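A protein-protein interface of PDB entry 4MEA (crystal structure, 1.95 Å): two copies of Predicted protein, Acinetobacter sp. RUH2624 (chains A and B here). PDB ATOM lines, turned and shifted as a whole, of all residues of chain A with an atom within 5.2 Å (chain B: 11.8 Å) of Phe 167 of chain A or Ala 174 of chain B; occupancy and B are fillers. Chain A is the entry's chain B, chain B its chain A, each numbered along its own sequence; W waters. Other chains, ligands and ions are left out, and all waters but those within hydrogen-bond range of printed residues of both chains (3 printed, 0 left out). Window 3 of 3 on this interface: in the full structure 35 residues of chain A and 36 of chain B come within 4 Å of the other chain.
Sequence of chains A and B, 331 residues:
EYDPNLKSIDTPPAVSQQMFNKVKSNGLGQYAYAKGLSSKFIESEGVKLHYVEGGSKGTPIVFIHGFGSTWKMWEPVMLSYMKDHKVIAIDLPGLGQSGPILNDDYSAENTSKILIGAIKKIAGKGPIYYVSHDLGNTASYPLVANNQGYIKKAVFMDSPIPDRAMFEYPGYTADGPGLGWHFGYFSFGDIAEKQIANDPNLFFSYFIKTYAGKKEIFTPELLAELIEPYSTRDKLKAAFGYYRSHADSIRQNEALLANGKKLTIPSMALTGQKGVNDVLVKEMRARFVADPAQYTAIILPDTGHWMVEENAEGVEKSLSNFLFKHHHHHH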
ATOM      1  N   ASP A 163     -21.329  -6.043 -11.481  1.00  0.00           N
ATOM      2  CA  ASP A 163     -21.802  -7.414 -11.478  1.00  0.00           C
ATOM      3  C   ASP A 163     -20.635  -8.313 -11.093  1.00  0.00           C
ATOM      4  O   ASP A 163     -19.580  -7.818 -10.678  1.00  0.00           O
ATOM      5  CB  ASP A 163     -22.444  -7.799 -12.824  1.00  0.00           C
ATOM      6  CG  ASP A 163     -21.432  -8.228 -13.878  1.00  0.00           C
ATOM      7  OD1 ASP A 163     -20.220  -7.928 -13.738  1.00  0.00           O
ATOM      8  OD2 ASP A 163     -21.865  -8.875 -14.863  1.00  0.00           O
ATOM      9  N   ARG A 164     -20.825  -9.621 -11.229  1.00  0.00           N
ATOM     10  CA  ARG A 164     -19.838 -10.604 -10.778  1.00  0.00           C
ATOM     11  C   ARG A 164     -18.438 -10.333 -11.328  1.00  0.00           C
ATOM     12  O   ARG A 164     -17.438 -10.614 -10.664  1.00  0.00           O
ATOM     13  CB  ARG A 164     -20.288 -12.010 -11.176  1.00  0.00           C
ATOM     14  CG  ARG A 164     -20.390 -12.200 -12.690  1.00  0.00           C
ATOM     15  CD  ARG A 164     -21.079 -13.518 -13.053  1.00  0.00           C
ATOM     16  NE  ARG A 164     -21.009 -13.763 -14.494  1.00  0.00           N
ATOM     17  CZ  ARG A 164     -21.732 -14.672 -15.139  1.00  0.00           C
ATOM     18  NH1 ARG A 164     -22.606 -15.425 -14.479  1.00  0.00           N
ATOM     19  NH2 ARG A 164     -21.588 -14.820 -16.451  1.00  0.00           N
ATOM     20  N   ALA A 165     -18.369  -9.793 -12.544  1.00  0.00           N
ATOM     21  CA  ALA A 165     -17.090  -9.555 -13.199  1.00  0.00           C
ATOM     22  C   ALA A 165     -16.270  -8.485 -12.479  1.00  0.00           C
ATOM     23  O   ALA A 165     -15.048  -8.423 -12.630  1.00  0.00           O
ATOM     24  CB  ALA A 165     -17.299  -9.168 -14.670  1.00  0.00           C
ATOM     25  N   MET A 166     -16.940  -7.651 -11.691  1.00  0.00           N
ATOM     26  CA  MET A 166     -16.251  -6.593 -10.954  1.00  0.00           C
ATOM     27  C   MET A 166     -15.406  -7.176  -9.802  1.00  0.00           C
ATOM     28  O   MET A 166     -14.509  -6.515  -9.277  1.00  0.00           O
ATOM     29  CB  MET A 166     -17.247  -5.533 -10.466  1.00  0.00           C
ATOM     30  CG  MET A 166     -16.598  -4.223  -9.988  1.00  0.00           C
ATOM     31  SD  MET A 166     -17.835  -2.941  -9.721  1.00  0.00           S
ATOM     32  CE  MET A 166     -18.050  -2.343 -11.397  1.00  0.00           C
ATOM     33  N   PHE A 167     -15.678  -8.428  -9.442  1.00  0.00           N
ATOM     34  CA  PHE A 167     -14.818  -9.185  -8.527  1.00  0.00           C
ATOM     35  C   PHE A 167     -13.686  -9.884  -9.308  1.00  0.00           C
ATOM     36  O   PHE A 167     -12.926 -10.678  -8.740  1.00  0.00           O
ATOM     37  CB  PHE A 167     -15.629 -10.246  -7.770  1.00  0.00           C
ATOM     38  CG  PHE A 167     -16.591  -9.688  -6.751  1.00  0.00           C
ATOM     39  CD1 PHE A 167     -16.290  -8.535  -6.037  1.00  0.00           C
ATOM     40  CD2 PHE A 167     -17.793 -10.335  -6.497  1.00  0.00           C
ATOM     41  CE1 PHE A 167     -17.181  -8.033  -5.082  1.00  0.00           C
ATOM     42  CE2 PHE A 167     -18.688  -9.839  -5.554  1.00  0.00           C
ATOM     43  CZ  PHE A 167     -18.379  -8.688  -4.841  1.00  0.00           C
ATOM     44  N   GLU A 168     -13.577  -9.591 -10.606  1.00  0.00           N
ATOM     45  CA  GLU A 168     -12.615 -10.286 -11.467  1.00  0.00           C
ATOM     46  C   GLU A 168     -11.668  -9.378 -12.267  1.00  0.00           C
ATOM     47  O   GLU A 168     -10.558  -9.796 -12.579  1.00  0.00           O
ATOM     48  CB  GLU A 168     -13.339 -11.228 -12.452  1.00  0.00           C
ATOM     49  CG  GLU A 168     -14.059 -12.396 -11.785  1.00  0.00           C
ATOM     50  CD  GLU A 168     -14.931 -13.187 -12.753  1.00  0.00           C
ATOM     51  OE1 GLU A 168     -15.231 -12.686 -13.861  1.00  0.00           O
ATOM     52  OE2 GLU A 168     -15.320 -14.318 -12.397  1.00  0.00           O
ATOM     53  N   TYR A 169     -12.102  -8.173 -12.638  1.00  0.00           N
ATOM     54  CA  TYR A 169     -11.242  -7.311 -13.464  1.00  0.00           C
ATOM     55  C   TYR A 169      -9.854  -7.250 -12.839  1.00  0.00           C
ATOM     56  O   TYR A 169      -9.716  -6.962 -11.661  1.00  0.00           O
ATOM     57  CB  TYR A 169     -11.801  -5.892 -13.592  1.00  0.00           C
ATOM     58  CG  TYR A 169     -13.207  -5.845 -14.158  1.00  0.00           C
ATOM     59  CD1 TYR A 169     -13.561  -6.607 -15.286  1.00  0.00           C
ATOM     60  CD2 TYR A 169     -14.183  -5.066 -13.562  1.00  0.00           C
ATOM     61  CE1 TYR A 169     -14.850  -6.581 -15.793  1.00  0.00           C
ATOM     62  CE2 TYR A 169     -15.485  -5.037 -14.061  1.00  0.00           C
ATOM     63  CZ  TYR A 169     -15.808  -5.790 -15.172  1.00  0.00           C
ATOM     64  OH  TYR A 169     -17.099  -5.739 -15.650  1.00  0.00           O
ATOM     65  N   ALA A 247     -19.164  -3.928  -3.539  1.00  0.00           N
ATOM     66  CA  ALA A 247     -19.538  -5.297  -3.198  1.00  0.00           C
ATOM     67  C   ALA A 247     -21.041  -5.395  -2.901  1.00  0.00           C
ATOM     68  O   ALA A 247     -21.702  -6.356  -3.324  1.00  0.00           O
ATOM     69  CB  ALA A 247     -18.702  -5.829  -2.020  1.00  0.00           C
ATOM     70  N   ILE A 250     -22.817  -5.033  -6.245  1.00  0.00           N
ATOM     71  CA  ILE A 250     -22.696  -6.250  -7.033  1.00  0.00           C
ATOM     72  C   ILE A 250     -23.723  -7.290  -6.567  1.00  0.00           C
ATOM     73  O   ILE A 250     -24.435  -7.898  -7.379  1.00  0.00           O
ATOM     74  CB  ILE A 250     -21.275  -6.826  -6.936  1.00  0.00           C
ATOM     75  CG1 ILE A 250     -20.275  -5.870  -7.601  1.00  0.00           C
ATOM     76  CG2 ILE A 250     -21.213  -8.226  -7.568  1.00  0.00           C
ATOM     77  CD1 ILE A 250     -18.850  -6.149  -7.220  1.00  0.00           C
ATOM     78  N   ARG A 251     -23.799  -7.496  -5.256  1.00  0.00           N
ATOM     79  CA  ARG A 251     -24.768  -8.443  -4.701  1.00  0.00           C
ATOM     80  C   ARG A 251     -26.201  -8.042  -5.034  1.00  0.00           C
ATOM     81  O   ARG A 251     -27.029  -8.897  -5.364  1.00  0.00           O
ATOM     82  CB  ARG A 251     -24.590  -8.598  -3.186  1.00  0.00           C
ATOM     83  CG  ARG A 251     -23.257  -9.266  -2.801  1.00  0.00           C
ATOM     84  CD  ARG A 251     -23.131  -9.525  -1.293  1.00  0.00           C
ATOM     85  NE  ARG A 251     -22.743  -8.348  -0.524  1.00  0.00           N
ATOM     86  CZ  ARG A 251     -21.497  -8.056  -0.142  1.00  0.00           C
ATOM     87  NH1 ARG A 251     -21.271  -6.955   0.575  1.00  0.00           N
ATOM     88  NH2 ARG A 251     -20.476  -8.854  -0.462  1.00  0.00           N
ATOM     89  N   GLU B   1      -5.178  -9.707   6.607  1.00  0.00           N
ATOM     90  CA  GLU B   1      -6.409  -9.659   5.814  1.00  0.00           C
ATOM     91  C   GLU B   1      -7.088  -8.283   5.886  1.00  0.00           C
ATOM     92  O   GLU B   1      -6.958  -7.567   6.895  1.00  0.00           O
ATOM     93  CB  GLU B   1      -7.384 -10.753   6.271  1.00  0.00           C
ATOM     94  CG  GLU B   1      -8.170 -10.426   7.548  1.00  0.00           C
ATOM     95  CD  GLU B   1      -7.393 -10.676   8.839  1.00  0.00           C
ATOM     96  OE1 GLU B   1      -6.194 -10.331   8.913  1.00  0.00           O
ATOM     97  OE2 GLU B   1      -7.989 -11.219   9.792  1.00  0.00           O
ATOM     98  N   TYR B   2      -7.808  -7.914   4.823  1.00  0.00           N
ATOM     99  CA  TYR B   2      -8.491  -6.620   4.798  1.00  0.00           C
ATOM    100  C   TYR B   2      -9.546  -6.518   5.901  1.00  0.00           C
ATOM    101  O   TYR B   2     -10.347  -7.432   6.094  1.00  0.00           O
ATOM    102  CB  TYR B   2      -9.120  -6.288   3.427  1.00  0.00           C
ATOM    103  CG  TYR B   2      -9.691  -4.876   3.411  1.00  0.00           C
ATOM    104  CD1 TYR B   2      -8.866  -3.778   3.192  1.00  0.00           C
ATOM    105  CD2 TYR B   2     -11.040  -4.639   3.669  1.00  0.00           C
ATOM    106  CE1 TYR B   2      -9.368  -2.482   3.205  1.00  0.00           C
ATOM    107  CE2 TYR B   2     -11.551  -3.342   3.685  1.00  0.00           C
ATOM    108  CZ  TYR B   2     -10.705  -2.263   3.453  1.00  0.00           C
ATOM    109  OH  TYR B   2     -11.184  -0.960   3.472  1.00  0.00           O
ATOM    110  N   ASP B   3      -9.517  -5.394   6.617  1.00  0.00           N
ATOM    111  CA  ASP B   3     -10.480  -5.089   7.674  1.00  0.00           C
ATOM    112  C   ASP B   3     -11.038  -3.684   7.455  1.00  0.00           C
ATOM    113  O   ASP B   3     -10.338  -2.690   7.678  1.00  0.00           O
ATOM    114  CB  ASP B   3      -9.804  -5.175   9.043  1.00  0.00           C
ATOM    115  CG  ASP B   3     -10.637  -4.559  10.149  1.00  0.00           C
ATOM    116  OD1 ASP B   3     -11.859  -4.366   9.950  1.00  0.00           O
ATOM    117  OD2 ASP B   3     -10.062  -4.271  11.221  1.00  0.00           O
ATOM    118  N   PRO B   4     -12.304  -3.592   7.019  1.00  0.00           N
ATOM    119  CA  PRO B   4     -12.900  -2.293   6.686  1.00  0.00           C
ATOM    120  C   PRO B   4     -12.942  -1.330   7.881  1.00  0.00           C
ATOM    121  O   PRO B   4     -13.110  -0.126   7.683  1.00  0.00           O
ATOM    122  CB  PRO B   4     -14.320  -2.666   6.232  1.00  0.00           C
ATOM    123  CG  PRO B   4     -14.589  -3.987   6.885  1.00  0.00           C
ATOM    124  CD  PRO B   4     -13.272  -4.695   6.877  1.00  0.00           C
ATOM    125  N   ALA B 165      -0.655 -15.638 -14.154  1.00  0.00           N
ATOM    126  CA  ALA B 165      -1.766 -15.375 -13.240  1.00  0.00           C
ATOM    127  C   ALA B 165      -1.696 -13.968 -12.625  1.00  0.00           C
ATOM    128  O   ALA B 165      -2.689 -13.446 -12.114  1.00  0.00           O
ATOM    129  CB  ALA B 165      -1.836 -16.445 -12.154  1.00  0.00           C
ATOM    130  N   PHE B 167      -1.438 -11.449 -14.288  1.00  0.00           N
ATOM    131  CA  PHE B 167      -2.252 -10.665 -15.207  1.00  0.00           C
ATOM    132  C   PHE B 167      -3.738 -10.906 -14.942  1.00  0.00           C
ATOM    133  O   PHE B 167      -4.606 -10.429 -15.691  1.00  0.00           O
ATOM    134  CB  PHE B 167      -1.938 -11.042 -16.659  1.00  0.00           C
ATOM    135  CG  PHE B 167      -0.592 -10.568 -17.135  1.00  0.00           C
ATOM    136  CD1 PHE B 167      -0.033  -9.409 -16.632  1.00  0.00           C
ATOM    137  CD2 PHE B 167       0.110 -11.286 -18.092  1.00  0.00           C
ATOM    138  CE1 PHE B 167       1.214  -8.965 -17.075  1.00  0.00           C
ATOM    139  CE2 PHE B 167       1.355 -10.847 -18.546  1.00  0.00           C
ATOM    140  CZ  PHE B 167       1.905  -9.689 -18.035  1.00  0.00           C
ATOM    141  N   GLU B 168      -4.030 -11.655 -13.884  1.00  0.00           N
ATOM    142  CA  GLU B 168      -5.408 -12.055 -13.591  1.00  0.00           C
ATOM    143  C   GLU B 168      -5.874 -11.721 -12.171  1.00  0.00           C
ATOM    144  O   GLU B 168      -7.079 -11.614 -11.929  1.00  0.00           O
ATOM    145  CB  GLU B 168      -5.590 -13.549 -13.869  1.00  0.00           C
ATOM    146  CG  GLU B 168      -5.401 -13.909 -15.337  1.00  0.00           C
ATOM    147  CD  GLU B 168      -5.221 -15.399 -15.557  1.00  0.00           C
ATOM    148  OE1 GLU B 168      -5.189 -16.152 -14.558  1.00  0.00           O
ATOM    149  OE2 GLU B 168      -5.105 -15.816 -16.731  1.00  0.00           O
ATOM    150  N   TYR B 169      -4.947 -11.556 -11.228  1.00  0.00           N
ATOM    151  CA  TYR B 169      -5.370 -11.284  -9.844  1.00  0.00           C
ATOM    152  C   TYR B 169      -6.276 -10.064  -9.834  1.00  0.00           C
ATOM    153  O   TYR B 169      -5.922  -9.023 -10.392  1.00  0.00           O
ATOM    154  CB  TYR B 169      -4.177 -11.069  -8.902  1.00  0.00           C
ATOM    155  CG  TYR B 169      -3.195 -12.220  -8.880  1.00  0.00           C
ATOM    156  CD1 TYR B 169      -3.636 -13.541  -8.814  1.00  0.00           C
ATOM    157  CD2 TYR B 169      -1.823 -11.984  -8.941  1.00  0.00           C
ATOM    158  CE1 TYR B 169      -2.729 -14.597  -8.804  1.00  0.00           C
ATOM    159  CE2 TYR B 169      -0.917 -13.022  -8.948  1.00  0.00           C
ATOM    160  CZ  TYR B 169      -1.372 -14.324  -8.875  1.00  0.00           C
ATOM    161  OH  TYR B 169      -0.459 -15.345  -8.870  1.00  0.00           O
ATOM    162  N   PRO B 170      -7.455 -10.184  -9.205  1.00  0.00           N
ATOM    163  CA  PRO B 170      -8.472  -9.131  -9.280  1.00  0.00           C
ATOM    164  C   PRO B 170      -8.156  -7.901  -8.420  1.00  0.00           C
ATOM    165  O   PRO B 170      -7.541  -8.007  -7.353  1.00  0.00           O
ATOM    166  CB  PRO B 170      -9.740  -9.831  -8.779  1.00  0.00           C
ATOM    167  CG  PRO B 170      -9.249 -10.890  -7.866  1.00  0.00           C
ATOM    168  CD  PRO B 170      -7.916 -11.352  -8.427  1.00  0.00           C
ATOM    169  N   GLY B 171      -8.571  -6.730  -8.885  1.00  0.00           N
ATOM    170  CA  GLY B 171      -8.363  -5.521  -8.108  1.00  0.00           C
ATOM    171  C   GLY B 171      -9.333  -5.427  -6.947  1.00  0.00           C
ATOM    172  O   GLY B 171      -9.055  -4.776  -5.932  1.00  0.00           O
ATOM    173  N   TYR B 172     -10.476  -6.090  -7.082  1.00  0.00           N
ATOM    174  CA  TYR B 172     -11.539  -5.939  -6.090  1.00  0.00           C
ATOM    175  C   TYR B 172     -12.258  -7.271  -5.862  1.00  0.00           C
ATOM    176  O   TYR B 172     -12.386  -8.083  -6.781  1.00  0.00           O
ATOM    177  CB  TYR B 172     -12.521  -4.848  -6.527  1.00  0.00           C
ATOM    178  CG  TYR B 172     -13.565  -4.477  -5.488  1.00  0.00           C
ATOM    179  CD1 TYR B 172     -13.203  -3.831  -4.309  1.00  0.00           C
ATOM    180  CD2 TYR B 172     -14.917  -4.771  -5.690  1.00  0.00           C
ATOM    181  CE1 TYR B 172     -14.151  -3.484  -3.364  1.00  0.00           C
ATOM    182  CE2 TYR B 172     -15.878  -4.422  -4.745  1.00  0.00           C
ATOM    183  CZ  TYR B 172     -15.481  -3.782  -3.580  1.00  0.00           C
ATOM    184  OH  TYR B 172     -16.412  -3.429  -2.629  1.00  0.00           O
ATOM    185  N   THR B 173     -12.701  -7.494  -4.630  1.00  0.00           N
ATOM    186  CA  THR B 173     -13.297  -8.767  -4.257  1.00  0.00           C
ATOM    187  C   THR B 173     -14.434  -8.550  -3.273  1.00  0.00           C
ATOM    188  O   THR B 173     -14.624  -7.448  -2.745  1.00  0.00           O
ATOM    189  CB  THR B 173     -12.271  -9.730  -3.599  1.00  0.00           C
ATOM    190  OG1 THR B 173     -11.967  -9.290  -2.266  1.00  0.00           O
ATOM    191  CG2 THR B 173     -10.988  -9.839  -4.429  1.00  0.00           C
ATOM    192  N   ALA B 174     -15.171  -9.618  -3.007  1.00  0.00           N
ATOM    193  CA  ALA B 174     -16.267  -9.566  -2.041  1.00  0.00           C
ATOM    194  C   ALA B 174     -15.726  -9.213  -0.660  1.00  0.00           C
ATOM    195  O   ALA B 174     -16.480  -8.855   0.236  1.00  0.00           O
ATOM    196  CB  ALA B 174     -17.009 -10.908  -1.997  1.00  0.00           C
ATOM    197  N   ASP B 175     -14.413  -9.321  -0.508  1.00  0.00           N
ATOM    198  CA  ASP B 175     -13.742  -9.032   0.757  1.00  0.00           C
ATOM    199  C   ASP B 175     -13.087  -7.645   0.750  1.00  0.00           C
ATOM    200  O   ASP B 175     -12.327  -7.303   1.654  1.00  0.00           O
ATOM    201  CB  ASP B 175     -12.680 -10.103   1.035  1.00  0.00           C
ATOM    202  CG  ASP B 175     -12.028  -9.939   2.395  1.00  0.00           C
ATOM    203  OD1 ASP B 175     -12.753  -9.654   3.374  1.00  0.00           O
ATOM    204  OD2 ASP B 175     -10.785 -10.086   2.480  1.00  0.00           O
ATOM    205  N   GLY B 176     -13.376  -6.853  -0.278  1.00  0.00           N
ATOM    206  CA  GLY B 176     -12.738  -5.557  -0.437  1.00  0.00           C
ATOM    207  C   GLY B 176     -11.568  -5.627  -1.404  1.00  0.00           C
ATOM    208  O   GLY B 176     -11.484  -6.547  -2.227  1.00  0.00           O
ATOM    209  N   PRO B 177     -10.648  -4.659  -1.310  1.00  0.00           N
ATOM    210  CA  PRO B 177      -9.512  -4.600  -2.246  1.00  0.00           C
ATOM    211  C   PRO B 177      -8.835  -5.961  -2.415  1.00  0.00           C
ATOM    212  O   PRO B 177      -8.586  -6.656  -1.430  1.00  0.00           O
ATOM    213  CB  PRO B 177      -8.564  -3.603  -1.573  1.00  0.00           C
ATOM    214  CG  PRO B 177      -9.495  -2.682  -0.826  1.00  0.00           C
ATOM    215  CD  PRO B 177     -10.593  -3.586  -0.298  1.00  0.00           C
ATOM    216  N   GLY B 178      -8.554  -6.342  -3.658  1.00  0.00           N
ATOM    217  CA  GLY B 178      -7.998  -7.654  -3.937  1.00  0.00           C
ATOM    218  C   GLY B 178      -6.493  -7.687  -4.116  1.00  0.00           C
ATOM    219  O   GLY B 178      -5.828  -6.637  -4.160  1.00  0.00           O
ATOM    220  N   LEU B 179      -5.959  -8.904  -4.215  1.00  0.00           N
ATOM    221  CA  LEU B 179      -4.522  -9.133  -4.416  1.00  0.00           C
ATOM    222  C   LEU B 179      -3.963  -8.360  -5.613  1.00  0.00           C
ATOM    223  O   LEU B 179      -2.789  -7.976  -5.636  1.00  0.00           O
ATOM    224  CB  LEU B 179      -4.258 -10.630  -4.610  1.00  0.00           C
ATOM    225  CG  LEU B 179      -2.815 -11.056  -4.884  1.00  0.00           C
ATOM    226  CD1 LEU B 179      -1.900 -10.648  -3.738  1.00  0.00           C
ATOM    227  CD2 LEU B 179      -2.744 -12.561  -5.132  1.00  0.00           C
ATOM    228  N   GLY B 180      -4.801  -8.140  -6.617  1.00  0.00           N
ATOM    229  CA  GLY B 180      -4.346  -7.482  -7.823  1.00  0.00           C
ATOM    230  C   GLY B 180      -4.151  -5.978  -7.742  1.00  0.00           C
ATOM    231  O   GLY B 180      -3.374  -5.426  -8.523  1.00  0.00           O
ATOM    232  N   TRP B 181      -4.848  -5.300  -6.830  1.00  0.00           N
ATOM    233  CA  TRP B 181      -4.923  -3.833  -6.917  1.00  0.00           C
ATOM    234  C   TRP B 181      -3.564  -3.147  -6.794  1.00  0.00           C
ATOM    235  O   TRP B 181      -3.261  -2.216  -7.552  1.00  0.00           O
ATOM    236  CB  TRP B 181      -5.966  -3.216  -5.954  1.00  0.00           C
ATOM    237  CG  TRP B 181      -5.480  -2.900  -4.547  1.00  0.00           C
ATOM    238  CD1 TRP B 181      -5.678  -3.658  -3.418  1.00  0.00           C
ATOM    239  CD2 TRP B 181      -4.743  -1.736  -4.120  1.00  0.00           C
ATOM    240  NE1 TRP B 181      -5.089  -3.052  -2.327  1.00  0.00           N
ATOM    241  CE2 TRP B 181      -4.516  -1.870  -2.728  1.00  0.00           C
ATOM    242  CE3 TRP B 181      -4.248  -0.600  -4.779  1.00  0.00           C
ATOM    243  CZ2 TRP B 181      -3.812  -0.919  -1.990  1.00  0.00           C
ATOM    244  CZ3 TRP B 181      -3.549   0.346  -4.040  1.00  0.00           C
ATOM    245  CH2 TRP B 181      -3.339   0.181  -2.657  1.00  0.00           C
HETATM  246  O   HOH W   1     -11.660  -6.388  -9.697  1.00  0.00           O
HETATM  247  O   HOH W   2     -18.393  -7.501   1.155  1.00  0.00           O
HETATM  248  O   HOH W   3      -9.455 -12.237 -12.837  1.00  0.00           O
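The backbone NH (N) of Gly 171 of chain B lies within hydrogen-bond range of the backbone carbonyl oxygen (O) of Tyr 169 of chain A, at 3.0 Å. The backbone NH (N) of Ala 247 of chain A sits at hydrogen-bond distance from the side-chain hydroxyl (OH) of Tyr 172 of chain B (2.9 Å). The backbone carbonyl oxygen (O) of Tyr 172 of chain B sits close to the backbone carbonyl oxygen (O) of Phe 167 of chain A, 3.3 Å away.
The side-chain hydroxyl (OG1) of Thr 173 of chain B sits close to the backbone NH (N) of Asp 175 of chain B (3.0 Å). OG1 of Thr 173 of chain B sits at hydrogen-bond distance from O of Gly 176 of chain B (2.8 Å). The backbone carbonyl oxygen (O) of Gly 171 of chain B is in hydrogen-bond range of the backbone NH (N) of Gly 178 of chain B, at 2.8 Å. The backbone carbonyl oxygen (O) of Pro 170 of chain B is in hydrogen-bond range of the backbone NH (N) of Gly 180 of chain B (2.8 Å).
Among the printed residues, merely in contact across the chains: Met 166 of chain A with Tyr 172 of chain B, Phe 167 of chain A with Pro 170 of chain B, Phe 167 of chain A with Thr 173 of chain B, Phe 167 of chain A with Ala 174 of chain B, Glu 168 of chain A with Glu 168 of chain B, Glu 168 of chain A with Pro 170 of chain B and Tyr 169 of chain A with Pro 170 of chain B.
Arg 164 of chain A touches none of the printed residues of chain B. Of chain B, only Tyr 172 comes within 4 Å of Met 166 of chain A. Glu 168 of chain A touches just these residues of chain B: Glu 168 and Pro 170. Of chain B, only Tyr 172 comes within 4 Å of Ala 247 of chain A. No residue of chain B comes within 4 Å of Ile 250 of chain A. Printed residues of chain A within 4 Å of Glu 168 of chain B: Glu 168. Printed residues of chain A within 4 Å of Gly 171 of chain B: Tyr 169 (3.0 Å). Of the printed residues of chain A, Tyr 172 of chain B touches Met 166 (3.6 Å), Phe 167 (3.2 Å) and Ala 247 (2.9 Å). Gly 176 of chain B touches none of the printed residues of chain A.
Of the 10 printed residues of chain A, 5 touch a printed residue of chain B. Hydrophobic or aromatic side chains of chain A within 4 Å of the printed part of chain B: Phe 167 and Ala 247. Along chain A the printed residues that touch a printed residue of chain B span positions 166 to 247. Of the 20 printed residues of chain B, 6 touch a printed residue of chain A. Printed residues of chain B that touch a printed residue of chain A: Glu 168, Pro 170, Gly 171, Tyr 172, Thr 173 and Ala 174. Hydrophobic or aromatic side chains of chain B within 4 Å of the printed part of chain A: Pro 170, Tyr 172 and Ala 174. Along chain B the printed residues that touch a printed residue of chain A span positions 168 to 174. Among the printed residues, no Asp or Glu carboxylate lies within 4 Å of a Lys or Arg side-chain nitrogen of the other chain.
Glu 168 of chain B touches its own counterpart, Glu 168 of chain A. Of the 10 pairs that touch across the chains among the printed residues, 1 has its exchanged pair printed and touching as well.
Water W2 lies within hydrogen-bond range of the backbone carbonyl oxygen (O) of Ala 174 of chain B (2.5 Å) and the guanidinium group (NH2) of Arg 251 of chain A (3.0 Å). Water W3 bridges the backbone carbonyl oxygen of Glu 168 of chain B and the backbone carbonyl oxygen of Glu 168 of chain A. Water W1 lies within hydrogen-bond range of O of Tyr 169 of chain A (2.8 Å), O of Met 166 of chain A (2.9 Å), N of Tyr 172 of chain B (2.9 Å) and N of Gly 171 of chain B (3.2 Å).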
